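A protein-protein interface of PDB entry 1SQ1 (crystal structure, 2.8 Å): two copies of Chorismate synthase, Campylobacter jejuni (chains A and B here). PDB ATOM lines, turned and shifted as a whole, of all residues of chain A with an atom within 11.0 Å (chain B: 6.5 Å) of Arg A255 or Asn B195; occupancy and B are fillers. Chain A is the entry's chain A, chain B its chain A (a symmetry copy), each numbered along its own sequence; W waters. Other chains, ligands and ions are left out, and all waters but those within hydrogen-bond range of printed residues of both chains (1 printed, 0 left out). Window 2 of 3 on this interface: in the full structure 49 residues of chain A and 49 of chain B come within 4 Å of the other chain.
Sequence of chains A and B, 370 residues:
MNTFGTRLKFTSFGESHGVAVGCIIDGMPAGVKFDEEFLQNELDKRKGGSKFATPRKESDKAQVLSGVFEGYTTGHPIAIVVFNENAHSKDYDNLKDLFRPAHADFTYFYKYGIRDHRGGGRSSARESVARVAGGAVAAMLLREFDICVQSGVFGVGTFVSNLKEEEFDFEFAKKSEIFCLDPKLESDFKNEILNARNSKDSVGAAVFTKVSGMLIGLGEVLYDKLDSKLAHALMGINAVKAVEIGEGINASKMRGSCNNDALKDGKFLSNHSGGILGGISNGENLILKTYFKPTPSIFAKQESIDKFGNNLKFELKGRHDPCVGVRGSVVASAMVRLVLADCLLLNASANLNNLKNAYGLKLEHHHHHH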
ATOM      1  N   GLU A 247      -2.551 -11.733 -22.712  1.00  0.00           N
ATOM      2  CA  GLU A 247      -3.362 -12.130 -21.567  1.00  0.00           C
ATOM      3  C   GLU A 247      -3.144 -13.586 -21.160  1.00  0.00           C
ATOM      4  O   GLU A 247      -3.363 -13.946 -20.006  1.00  0.00           O
ATOM      5  CB  GLU A 247      -4.855 -11.902 -21.840  1.00  0.00           C
ATOM      6  CG  GLU A 247      -5.323 -10.467 -21.653  1.00  0.00           C
ATOM      7  CD  GLU A 247      -4.935  -9.869 -20.300  1.00  0.00           C
ATOM      8  OE1 GLU A 247      -5.354 -10.402 -19.243  1.00  0.00           O
ATOM      9  OE2 GLU A 247      -4.203  -8.852 -20.301  1.00  0.00           O
ATOM     10  N   GLY A 248      -2.727 -14.420 -22.109  1.00  0.00           N
ATOM     11  CA  GLY A 248      -2.489 -15.824 -21.816  1.00  0.00           C
ATOM     12  C   GLY A 248      -3.644 -16.626 -21.226  1.00  0.00           C
ATOM     13  O   GLY A 248      -4.789 -16.556 -21.680  1.00  0.00           O
ATOM     14  N   ILE A 249      -3.338 -17.409 -20.201  1.00  0.00           N
ATOM     15  CA  ILE A 249      -4.350 -18.231 -19.554  1.00  0.00           C
ATOM     16  C   ILE A 249      -5.508 -17.365 -19.072  1.00  0.00           C
ATOM     17  O   ILE A 249      -6.663 -17.781 -19.116  1.00  0.00           O
ATOM     18  CB  ILE A 249      -3.749 -18.998 -18.359  1.00  0.00           C
ATOM     19  CG1 ILE A 249      -2.690 -19.978 -18.862  1.00  0.00           C
ATOM     20  CG2 ILE A 249      -4.833 -19.746 -17.613  1.00  0.00           C
ATOM     21  CD1 ILE A 249      -1.976 -20.707 -17.761  1.00  0.00           C
ATOM     22  N   ASN A 250      -5.184 -16.155 -18.621  1.00  0.00           N
ATOM     23  CA  ASN A 250      -6.182 -15.222 -18.114  1.00  0.00           C
ATOM     24  C   ASN A 250      -7.204 -14.801 -19.163  1.00  0.00           C
ATOM     25  O   ASN A 250      -8.356 -14.500 -18.842  1.00  0.00           O
ATOM     26  CB  ASN A 250      -5.502 -13.980 -17.534  1.00  0.00           C
ATOM     27  CG  ASN A 250      -6.496 -13.023 -16.896  1.00  0.00           C
ATOM     28  OD1 ASN A 250      -6.697 -11.911 -17.383  1.00  0.00           O
ATOM     29  ND2 ASN A 250      -7.132 -13.458 -15.806  1.00  0.00           N
ATOM     30  N   ALA A 251      -6.795 -14.769 -20.419  1.00  0.00           N
ATOM     31  CA  ALA A 251      -7.742 -14.378 -21.439  1.00  0.00           C
ATOM     32  C   ALA A 251      -8.880 -15.382 -21.455  1.00  0.00           C
ATOM     33  O   ALA A 251      -9.970 -15.062 -21.899  1.00  0.00           O
ATOM     34  CB  ALA A 251      -7.071 -14.321 -22.808  1.00  0.00           C
ATOM     35  N   SER A 252      -8.646 -16.591 -20.957  1.00  0.00           N
ATOM     36  CA  SER A 252      -9.699 -17.603 -20.986  1.00  0.00           C
ATOM     37  C   SER A 252     -10.836 -17.309 -20.008  1.00  0.00           C
ATOM     38  O   SER A 252     -11.976 -17.740 -20.211  1.00  0.00           O
ATOM     39  CB  SER A 252      -9.113 -18.983 -20.696  1.00  0.00           C
ATOM     40  OG  SER A 252      -8.678 -19.083 -19.356  1.00  0.00           O
ATOM     41  N   LYS A 253     -10.515 -16.550 -18.962  1.00  0.00           N
ATOM     42  CA  LYS A 253     -11.460 -16.174 -17.920  1.00  0.00           C
ATOM     43  C   LYS A 253     -12.089 -14.809 -18.145  1.00  0.00           C
ATOM     44  O   LYS A 253     -12.819 -14.317 -17.289  1.00  0.00           O
ATOM     45  CB  LYS A 253     -10.740 -16.180 -16.572  1.00  0.00           C
ATOM     46  CG  LYS A 253     -10.305 -17.564 -16.139  1.00  0.00           C
ATOM     47  CD  LYS A 253      -9.559 -17.539 -14.835  1.00  0.00           C
ATOM     48  CE  LYS A 253      -8.175 -16.982 -15.026  1.00  0.00           C
ATOM     49  NZ  LYS A 253      -7.444 -17.029 -13.740  1.00  0.00           N
ATOM     50  N   MET A 254     -11.809 -14.194 -19.290  1.00  0.00           N
ATOM     51  CA  MET A 254     -12.344 -12.870 -19.610  1.00  0.00           C
ATOM     52  C   MET A 254     -13.541 -12.914 -20.542  1.00  0.00           C
ATOM     53  O   MET A 254     -13.942 -13.970 -21.011  1.00  0.00           O
ATOM     54  CB  MET A 254     -11.254 -12.006 -20.255  1.00  0.00           C
ATOM     55  CG  MET A 254     -10.240 -11.424 -19.289  1.00  0.00           C
ATOM     56  SD  MET A 254      -8.687 -10.690 -20.213  1.00  0.00           S
ATOM     57  CE  MET A 254      -9.311  -8.900 -20.605  1.00  0.00           C
ATOM     58  N   ARG A 255     -14.124 -11.753 -20.795  1.00  0.00           N
ATOM     59  CA  ARG A 255     -15.237 -11.662 -21.723  1.00  0.00           C
ATOM     60  C   ARG A 255     -14.812 -10.815 -22.908  1.00  0.00           C
ATOM     61  O   ARG A 255     -13.980  -9.925 -22.771  1.00  0.00           O
ATOM     62  CB  ARG A 255     -16.451 -11.031 -21.063  1.00  0.00           C
ATOM     63  CG  ARG A 255     -17.053 -11.876 -19.995  1.00  0.00           C
ATOM     64  CD  ARG A 255     -18.523 -11.608 -19.928  1.00  0.00           C
ATOM     65  NE  ARG A 255     -19.199 -12.624 -19.138  1.00  0.00           N
ATOM     66  CZ  ARG A 255     -20.514 -12.688 -18.985  1.00  0.00           C
ATOM     67  NH1 ARG A 255     -21.296 -11.792 -19.572  1.00  0.00           N
ATOM     68  NH2 ARG A 255     -21.041 -13.647 -18.242  1.00  0.00           N
ATOM     69  N   GLY A 256     -15.389 -11.091 -24.069  1.00  0.00           N
ATOM     70  CA  GLY A 256     -15.045 -10.339 -25.261  1.00  0.00           C
ATOM     71  C   GLY A 256     -14.941  -8.836 -25.043  1.00  0.00           C
ATOM     72  O   GLY A 256     -14.023  -8.188 -25.558  1.00  0.00           O
ATOM     73  N   SER A 257     -15.878  -8.284 -24.278  1.00  0.00           N
ATOM     74  CA  SER A 257     -15.912  -6.855 -23.999  1.00  0.00           C
ATOM     75  C   SER A 257     -14.718  -6.331 -23.205  1.00  0.00           C
ATOM     76  O   SER A 257     -14.536  -5.117 -23.102  1.00  0.00           O
ATOM     77  CB  SER A 257     -17.199  -6.511 -23.254  1.00  0.00           C
ATOM     78  OG  SER A 257     -17.250  -7.172 -22.006  1.00  0.00           O
ATOM     79  N   CYS A 258     -13.908  -7.231 -22.648  1.00  0.00           N
ATOM     80  CA  CYS A 258     -12.738  -6.830 -21.859  1.00  0.00           C
ATOM     81  C   CYS A 258     -11.400  -7.193 -22.525  1.00  0.00           C
ATOM     82  O   CYS A 258     -10.369  -6.586 -22.222  1.00  0.00           O
ATOM     83  CB  CYS A 258     -12.794  -7.469 -20.464  1.00  0.00           C
ATOM     84  SG  CYS A 258     -14.357  -7.218 -19.565  1.00  0.00           S
ATOM     85  N   ASN A 259     -11.424  -8.171 -23.432  1.00  0.00           N
ATOM     86  CA  ASN A 259     -10.214  -8.611 -24.125  1.00  0.00           C
ATOM     87  C   ASN A 259     -10.009  -7.868 -25.439  1.00  0.00           C
ATOM     88  O   ASN A 259      -8.880  -7.652 -25.878  1.00  0.00           O
ATOM     89  CB  ASN A 259     -10.284 -10.113 -24.409  1.00  0.00           C
ATOM     90  CG  ASN A 259      -8.921 -10.760 -24.414  1.00  0.00           C
ATOM     91  OD1 ASN A 259      -8.166 -10.627 -23.457  1.00  0.00           O
ATOM     92  ND2 ASN A 259      -8.600 -11.464 -25.484  1.00  0.00           N
ATOM     93  N   ASN A 260     -11.121  -7.486 -26.059  1.00  0.00           N
ATOM     94  CA  ASN A 260     -11.117  -6.769 -27.329  1.00  0.00           C
ATOM     95  C   ASN A 260     -10.175  -5.573 -27.341  1.00  0.00           C
ATOM     96  O   ASN A 260     -10.221  -4.725 -26.456  1.00  0.00           O
ATOM     97  CB  ASN A 260     -12.550  -6.317 -27.658  1.00  0.00           C
ATOM     98  CG  ASN A 260     -12.598  -5.153 -28.643  1.00  0.00           C
ATOM     99  OD1 ASN A 260     -11.975  -5.192 -29.706  1.00  0.00           O
ATOM    100  ND2 ASN A 260     -13.356  -4.114 -28.295  1.00  0.00           N
ATOM    101  N   ASP A 261      -9.311  -5.519 -28.348  1.00  0.00           N
ATOM    102  CA  ASP A 261      -8.375  -4.409 -28.499  1.00  0.00           C
ATOM    103  C   ASP A 261      -8.831  -3.581 -29.698  1.00  0.00           C
ATOM    104  O   ASP A 261      -8.675  -4.011 -30.838  1.00  0.00           O
ATOM    105  CB  ASP A 261      -6.954  -4.927 -28.754  1.00  0.00           C
ATOM    106  CG  ASP A 261      -6.423  -5.771 -27.615  1.00  0.00           C
ATOM    107  OD1 ASP A 261      -6.522  -5.330 -26.453  1.00  0.00           O
ATOM    108  OD2 ASP A 261      -5.894  -6.870 -27.878  1.00  0.00           O
ATOM    109  N   SER A 270      -5.761  -1.006 -26.293  1.00  0.00           N
ATOM    110  CA  SER A 270      -5.256  -2.011 -25.358  1.00  0.00           C
ATOM    111  C   SER A 270      -4.390  -3.034 -26.097  1.00  0.00           C
ATOM    112  O   SER A 270      -4.450  -3.117 -27.320  1.00  0.00           O
ATOM    113  CB  SER A 270      -6.443  -2.705 -24.686  1.00  0.00           C
ATOM    114  OG  SER A 270      -7.477  -2.950 -25.635  1.00  0.00           O
ATOM    115  N   HIS A 272      -4.183  -6.593 -25.223  1.00  0.00           N
ATOM    116  CA  HIS A 272      -4.478  -7.897 -24.653  1.00  0.00           C
ATOM    117  C   HIS A 272      -3.990  -9.022 -25.536  1.00  0.00           C
ATOM    118  O   HIS A 272      -3.575 -10.074 -25.048  1.00  0.00           O
ATOM    119  CB  HIS A 272      -5.974  -8.039 -24.442  1.00  0.00           C
ATOM    120  CG  HIS A 272      -6.520  -7.109 -23.408  1.00  0.00           C
ATOM    121  ND1 HIS A 272      -6.022  -7.055 -22.124  1.00  0.00           N
ATOM    122  CD2 HIS A 272      -7.523  -6.200 -23.464  1.00  0.00           C
ATOM    123  CE1 HIS A 272      -6.694  -6.155 -21.433  1.00  0.00           C
ATOM    124  NE2 HIS A 272      -7.611  -5.621 -22.221  1.00  0.00           N
ATOM    125  N   SER A 273      -4.042  -8.782 -26.839  1.00  0.00           N
ATOM    126  CA  SER A 273      -3.624  -9.749 -27.841  1.00  0.00           C
ATOM    127  C   SER A 273      -2.149 -10.137 -27.758  1.00  0.00           C
ATOM    128  O   SER A 273      -1.746 -11.166 -28.284  1.00  0.00           O
ATOM    129  CB  SER A 273      -3.913  -9.191 -29.231  1.00  0.00           C
ATOM    130  OG  SER A 273      -3.151  -8.015 -29.451  1.00  0.00           O
ATOM    131  N   GLY B 157     -15.112 -18.875 -18.463  1.00  0.00           N
ATOM    132  CA  GLY B 157     -15.199 -17.635 -17.726  1.00  0.00           C
ATOM    133  C   GLY B 157     -14.446 -17.773 -16.421  1.00  0.00           C
ATOM    134  O   GLY B 157     -13.354 -18.332 -16.385  1.00  0.00           O
ATOM    135  N   LYS B 190     -22.788 -23.496 -18.840  1.00  0.00           N
ATOM    136  CA  LYS B 190     -23.945 -23.202 -19.692  1.00  0.00           C
ATOM    137  C   LYS B 190     -24.516 -21.819 -19.442  1.00  0.00           C
ATOM    138  O   LYS B 190     -24.752 -21.040 -20.368  1.00  0.00           O
ATOM    139  CB  LYS B 190     -25.041 -24.244 -19.466  1.00  0.00           C
ATOM    140  CG  LYS B 190     -24.669 -25.629 -19.942  1.00  0.00           C
ATOM    141  CD  LYS B 190     -25.803 -26.602 -19.744  1.00  0.00           C
ATOM    142  CE  LYS B 190     -25.457 -27.960 -20.321  1.00  0.00           C
ATOM    143  NZ  LYS B 190     -26.573 -28.936 -20.130  1.00  0.00           N
ATOM    144  N   ASN B 191     -24.748 -21.543 -18.167  1.00  0.00           N
ATOM    145  CA  ASN B 191     -25.283 -20.276 -17.711  1.00  0.00           C
ATOM    146  C   ASN B 191     -24.340 -19.155 -18.130  1.00  0.00           C
ATOM    147  O   ASN B 191     -24.771 -18.175 -18.741  1.00  0.00           O
ATOM    148  CB  ASN B 191     -25.423 -20.328 -16.190  1.00  0.00           C
ATOM    149  CG  ASN B 191     -25.398 -18.966 -15.558  1.00  0.00           C
ATOM    150  OD1 ASN B 191     -24.630 -18.718 -14.625  1.00  0.00           O
ATOM    151  ND2 ASN B 191     -26.234 -18.069 -16.059  1.00  0.00           N
ATOM    152  N   GLU B 192     -23.054 -19.312 -17.810  1.00  0.00           N
ATOM    153  CA  GLU B 192     -22.031 -18.317 -18.144  1.00  0.00           C
ATOM    154  C   GLU B 192     -22.026 -18.022 -19.639  1.00  0.00           C
ATOM    155  O   GLU B 192     -21.883 -16.872 -20.052  1.00  0.00           O
ATOM    156  CB  GLU B 192     -20.644 -18.815 -17.709  1.00  0.00           C
ATOM    157  CG  GLU B 192     -19.476 -17.971 -18.216  1.00  0.00           C
ATOM    158  CD  GLU B 192     -19.408 -16.604 -17.567  1.00  0.00           C
ATOM    159  OE1 GLU B 192     -18.520 -15.802 -17.931  1.00  0.00           O
ATOM    160  OE2 GLU B 192     -20.239 -16.328 -16.683  1.00  0.00           O
ATOM    161  N   ILE B 193     -22.186 -19.071 -20.443  1.00  0.00           N
ATOM    162  CA  ILE B 193     -22.208 -18.942 -21.895  1.00  0.00           C
ATOM    163  C   ILE B 193     -23.488 -18.240 -22.342  1.00  0.00           C
ATOM    164  O   ILE B 193     -23.450 -17.271 -23.104  1.00  0.00           O
ATOM    165  CB  ILE B 193     -22.109 -20.336 -22.576  1.00  0.00           C
ATOM    166  CG1 ILE B 193     -20.691 -20.892 -22.389  1.00  0.00           C
ATOM    167  CG2 ILE B 193     -22.485 -20.236 -24.058  1.00  0.00           C
ATOM    168  CD1 ILE B 193     -20.481 -22.283 -22.964  1.00  0.00           C
ATOM    169  N   LEU B 194     -24.621 -18.740 -21.866  1.00  0.00           N
ATOM    170  CA  LEU B 194     -25.913 -18.155 -22.198  1.00  0.00           C
ATOM    171  C   LEU B 194     -25.864 -16.665 -21.814  1.00  0.00           C
ATOM    172  O   LEU B 194     -26.159 -15.786 -22.634  1.00  0.00           O
ATOM    173  CB  LEU B 194     -27.018 -18.875 -21.417  1.00  0.00           C
ATOM    174  CG  LEU B 194     -28.308 -19.245 -22.153  1.00  0.00           C
ATOM    175  CD1 LEU B 194     -29.204 -20.031 -21.216  1.00  0.00           C
ATOM    176  CD2 LEU B 194     -29.021 -18.001 -22.648  1.00  0.00           C
ATOM    177  N   ASN B 195     -25.476 -16.381 -20.571  1.00  0.00           N
ATOM    178  CA  ASN B 195     -25.390 -15.005 -20.113  1.00  0.00           C
ATOM    179  C   ASN B 195     -24.548 -14.191 -21.081  1.00  0.00           C
ATOM    180  O   ASN B 195     -24.935 -13.097 -21.479  1.00  0.00           O
ATOM    181  CB  ASN B 195     -24.769 -14.938 -18.719  1.00  0.00           C
ATOM    182  CG  ASN B 195     -24.846 -13.548 -18.119  1.00  0.00           C
ATOM    183  OD1 ASN B 195     -25.930 -13.057 -17.814  1.00  0.00           O
ATOM    184  ND2 ASN B 195     -23.697 -12.903 -17.958  1.00  0.00           N
ATOM    185  N   ALA B 196     -23.395 -14.735 -21.457  1.00  0.00           N
ATOM    186  CA  ALA B 196     -22.498 -14.058 -22.384  1.00  0.00           C
ATOM    187  C   ALA B 196     -23.172 -13.848 -23.739  1.00  0.00           C
ATOM    188  O   ALA B 196     -22.910 -12.855 -24.423  1.00  0.00           O
ATOM    189  CB  ALA B 196     -21.218 -14.859 -22.553  1.00  0.00           C
ATOM    190  N   ARG B 197     -24.049 -14.772 -24.125  1.00  0.00           N
ATOM    191  CA  ARG B 197     -24.751 -14.659 -25.402  1.00  0.00           C
ATOM    192  C   ARG B 197     -25.748 -13.512 -25.357  1.00  0.00           C
ATOM    193  O   ARG B 197     -25.568 -12.499 -26.034  1.00  0.00           O
ATOM    194  CB  ARG B 197     -25.487 -15.964 -25.747  1.00  0.00           C
ATOM    195  CG  ARG B 197     -26.182 -15.928 -27.107  1.00  0.00           C
ATOM    196  CD  ARG B 197     -26.539 -17.323 -27.611  1.00  0.00           C
ATOM    197  NE  ARG B 197     -27.592 -17.979 -26.835  1.00  0.00           N
ATOM    198  CZ  ARG B 197     -28.855 -17.555 -26.763  1.00  0.00           C
ATOM    199  NH1 ARG B 197     -29.238 -16.462 -27.421  1.00  0.00           N
ATOM    200  NH2 ARG B 197     -29.745 -18.232 -26.044  1.00  0.00           N
ATOM    201  N   ASN B 198     -26.792 -13.676 -24.544  1.00  0.00           N
ATOM    202  CA  ASN B 198     -27.835 -12.665 -24.402  1.00  0.00           C
ATOM    203  C   ASN B 198     -27.243 -11.262 -24.264  1.00  0.00           C
ATOM    204  O   ASN B 198     -27.785 -10.300 -24.815  1.00  0.00           O
ATOM    205  CB  ASN B 198     -28.709 -12.978 -23.189  1.00  0.00           C
ATOM    206  CG  ASN B 198     -29.307 -14.370 -23.251  1.00  0.00           C
ATOM    207  OD1 ASN B 198     -29.571 -14.893 -24.336  1.00  0.00           O
ATOM    208  ND2 ASN B 198     -29.536 -14.975 -22.090  1.00  0.00           N
ATOM    209  N   SER B 199     -26.130 -11.153 -23.537  1.00  0.00           N
ATOM    210  CA  SER B 199     -25.463  -9.872 -23.332  1.00  0.00           C
ATOM    211  C   SER B 199     -24.821  -9.368 -24.612  1.00  0.00           C
ATOM    212  O   SER B 199     -24.238  -8.280 -24.622  1.00  0.00           O
ATOM    213  CB  SER B 199     -24.363  -9.996 -22.276  1.00  0.00           C
ATOM    214  OG  SER B 199     -24.890 -10.239 -20.994  1.00  0.00           O
ATOM    215  N   LYS B 200     -24.926 -10.153 -25.683  1.00  0.00           N
ATOM    216  CA  LYS B 200     -24.301  -9.805 -26.957  1.00  0.00           C
ATOM    217  C   LYS B 200     -22.819  -9.613 -26.671  1.00  0.00           C
ATOM    218  O   LYS B 200     -22.238  -8.576 -26.988  1.00  0.00           O
ATOM    219  CB  LYS B 200     -24.886  -8.509 -27.541  1.00  0.00           C
ATOM    220  CG  LYS B 200     -26.299  -8.638 -28.090  1.00  0.00           C
ATOM    221  CD  LYS B 200     -26.756  -7.358 -28.787  1.00  0.00           C
ATOM    222  CE  LYS B 200     -25.934  -7.070 -30.045  1.00  0.00           C
ATOM    223  NZ  LYS B 200     -26.378  -5.827 -30.763  1.00  0.00           N
ATOM    224  N   ASP B 201     -22.219 -10.613 -26.033  1.00  0.00           N
ATOM    225  CA  ASP B 201     -20.800 -10.568 -25.690  1.00  0.00           C
ATOM    226  C   ASP B 201     -20.264 -11.991 -25.829  1.00  0.00           C
ATOM    227  O   ASP B 201     -20.999 -12.901 -26.221  1.00  0.00           O
ATOM    228  CB  ASP B 201     -20.624 -10.068 -24.248  1.00  0.00           C
ATOM    229  CG  ASP B 201     -19.225  -9.543 -23.972  1.00  0.00           C
ATOM    230  OD1 ASP B 201     -18.956  -9.182 -22.798  1.00  0.00           O
ATOM    231  OD2 ASP B 201     -18.406  -9.486 -24.924  1.00  0.00           O
ATOM    232  N   SER B 202     -18.989 -12.190 -25.517  1.00  0.00           N
ATOM    233  CA  SER B 202     -18.396 -13.516 -25.615  1.00  0.00           C
ATOM    234  C   SER B 202     -17.622 -13.818 -24.338  1.00  0.00           C
ATOM    235  O   SER B 202     -17.484 -12.947 -23.470  1.00  0.00           O
ATOM    236  CB  SER B 202     -17.455 -13.579 -26.811  1.00  0.00           C
ATOM    237  OG  SER B 202     -16.353 -12.714 -26.607  1.00  0.00           O
ATOM    238  N   VAL B 203     -17.123 -15.048 -24.224  1.00  0.00           N
ATOM    239  CA  VAL B 203     -16.356 -15.465 -23.049  1.00  0.00           C
ATOM    240  C   VAL B 203     -15.313 -16.513 -23.398  1.00  0.00           C
ATOM    241  O   VAL B 203     -15.558 -17.373 -24.235  1.00  0.00           O
ATOM    242  CB  VAL B 203     -17.272 -16.050 -21.961  1.00  0.00           C
ATOM    243  CG1 VAL B 203     -18.090 -17.177 -22.541  1.00  0.00           C
ATOM    244  CG2 VAL B 203     -16.435 -16.544 -20.788  1.00  0.00           C
ATOM    245  N   GLY B 204     -14.155 -16.439 -22.743  1.00  0.00           N
ATOM    246  CA  GLY B 204     -13.091 -17.400 -22.994  1.00  0.00           C
ATOM    247  C   GLY B 204     -13.393 -18.786 -22.447  1.00  0.00           C
ATOM    248  O   GLY B 204     -14.466 -19.009 -21.881  1.00  0.00           O
ATOM    249  N   PRO B 294     -12.001 -15.001 -25.384  1.00  0.00           N
ATOM    250  CA  PRO B 294     -13.379 -14.804 -25.830  1.00  0.00           C
ATOM    251  C   PRO B 294     -13.419 -14.377 -27.294  1.00  0.00           C
ATOM    252  O   PRO B 294     -12.595 -13.581 -27.754  1.00  0.00           O
ATOM    253  CB  PRO B 294     -13.902 -13.727 -24.882  1.00  0.00           C
ATOM    254  CG  PRO B 294     -12.663 -12.991 -24.481  1.00  0.00           C
ATOM    255  CD  PRO B 294     -11.679 -14.098 -24.269  1.00  0.00           C
ATOM    256  N   THR B 295     -14.377 -14.940 -28.018  1.00  0.00           N
ATOM    257  CA  THR B 295     -14.589 -14.661 -29.434  1.00  0.00           C
ATOM    258  C   THR B 295     -14.580 -13.160 -29.692  1.00  0.00           C
ATOM    259  O   THR B 295     -15.297 -12.411 -29.031  1.00  0.00           O
ATOM    260  CB  THR B 295     -15.947 -15.195 -29.872  1.00  0.00           C
ATOM    261  OG1 THR B 295     -16.298 -16.324 -29.062  1.00  0.00           O
ATOM    262  CG2 THR B 295     -15.901 -15.603 -31.325  1.00  0.00           C
HETATM  263  O   HOH W   1     -21.066  -9.405 -20.611  1.00  0.00           O
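The backbone NH (N) of Gly A256 lies within hydrogen-bond range of the backbone carbonyl oxygen (O) of Ser B202 (2.9 Å).
NH2 of Arg A255 is in salt-bridge range of OE2 of Glu B192, at 3.2 Å.
The side-chain amide nitrogen of Asn B195 sits close to the guanidinium group of Arg A255 (2.8 Å).
O of Met A254 lies within hydrogen-bond range of N of Gly B204 (3.0 Å).
The side-chain carboxylate (OD1) of Asp B201 sits at hydrogen-bond distance from the side-chain hydroxyl (OG) of Ser A257, 2.8 Å away.
O of Gly B204 sits close to O of Ser A252 (3.3 Å).
The side-chain amide oxygen (OD1) of Asn A250 sits close to the side-chain sulfur (SD) of Met A254, 3.7 Å away.
N of Gly B157 sits at hydrogen-bond distance from O of Gly B204, 3.5 Å away.
The backbone carbonyl oxygen (O) of Thr B295 sits at hydrogen-bond distance from the side-chain hydroxyl (OG) of Ser B202, 2.7 Å away.
OG of Ser A257 sits close to SG of Cys A258 (3.8 Å).
The backbone carbonyl oxygen of Ile A249 is in hydrogen-bond range of the side-chain hydroxyl of Ser A252 (2.4 Å).
The side-chain amide oxygen (OD1) of Asn A259 sits close to the side-chain sulfur (SD) of Met A254, 3.3 Å away.
Among the printed residues, merely in contact across the chains: Ala A251 with Pro B294, Arg A255 with Ser B202, Gly A256 with Pro B294, Lys A253 with Gly B157, Arg A255 with Pro B294, Gly A256 with Asp B201, Met A254 with Val B203, Arg A255 with Asp B201, Asn A259 with Pro B294, Ser A252 with Gly B157, Arg A255 with Ala B196 and Met A254 with Pro B294.
Of the printed residues of chain B, Arg A255 touches Glu B192 (3.2 Å), Asn B195 (2.8 Å), Ala B196 (3.8 Å), Asp B201 (3.6 Å), Ser B202 (3.1 Å) and Pro B294 (3.4 Å).
No residue of chain A comes within 4 Å of Leu B194.
Of chain A, only Arg A255 (3.8 Å) comes within 4 Å of Ala B196.
Asn B198 touches none of the printed residues of chain A.
No residue of chain A comes within 4 Å of Ser B199.
Asp B201 touches just these residues of chain A: Arg A255 (3.6 Å), Gly A256 (3.5 Å) and Ser A257 (2.8 Å).
Val B203 touches one residue of chain A.
Of the printed residues of chain A, Pro B294 touches Ala A251, Met A254, Arg A255, Gly A256 and Asn A259.
Printed residues of chain B within 4 Å of Ser A252: Gly B157 (3.8 Å) and Gly B204 (2.8 Å).
Printed residues of chain B within 4 Å of Asn A259: Pro B294.
Of the printed residues of chain B, Lys A253 touches Gly B157 (3.2 Å).
Ser A270 touches none of the printed residues of chain B.
The nearest residue of chain A that does not touch Asn B195 is Ser A257 (9.5 Å).
The nearest printed residue of chain A that does not touch Gly B204 is Ala A251 (4.1 Å).
Of the 18 printed residues of chain B, 9 touch a printed residue of chain A.
Printed residues of chain B that touch a printed residue of chain A: Gly B157, Glu B192, Asn B195, Ala B196, Asp B201, Ser B202, Val B203, Gly B204 and Pro B294.
Hydrophobic or aromatic side chains of chain B that line the printed part of chain A: Val B203 and Pro B294.
Among the printed residues, 18 pairs touch across the chains.
No position is printed for both chains.
Of the 18 pairs that touch across the chains among the printed residues, none has its exchanged pair printed and touching as well.
Water W1 bridges NH1 of Arg A255 (2.6 Å) and OD1 of Asp B201 (3.0 Å).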
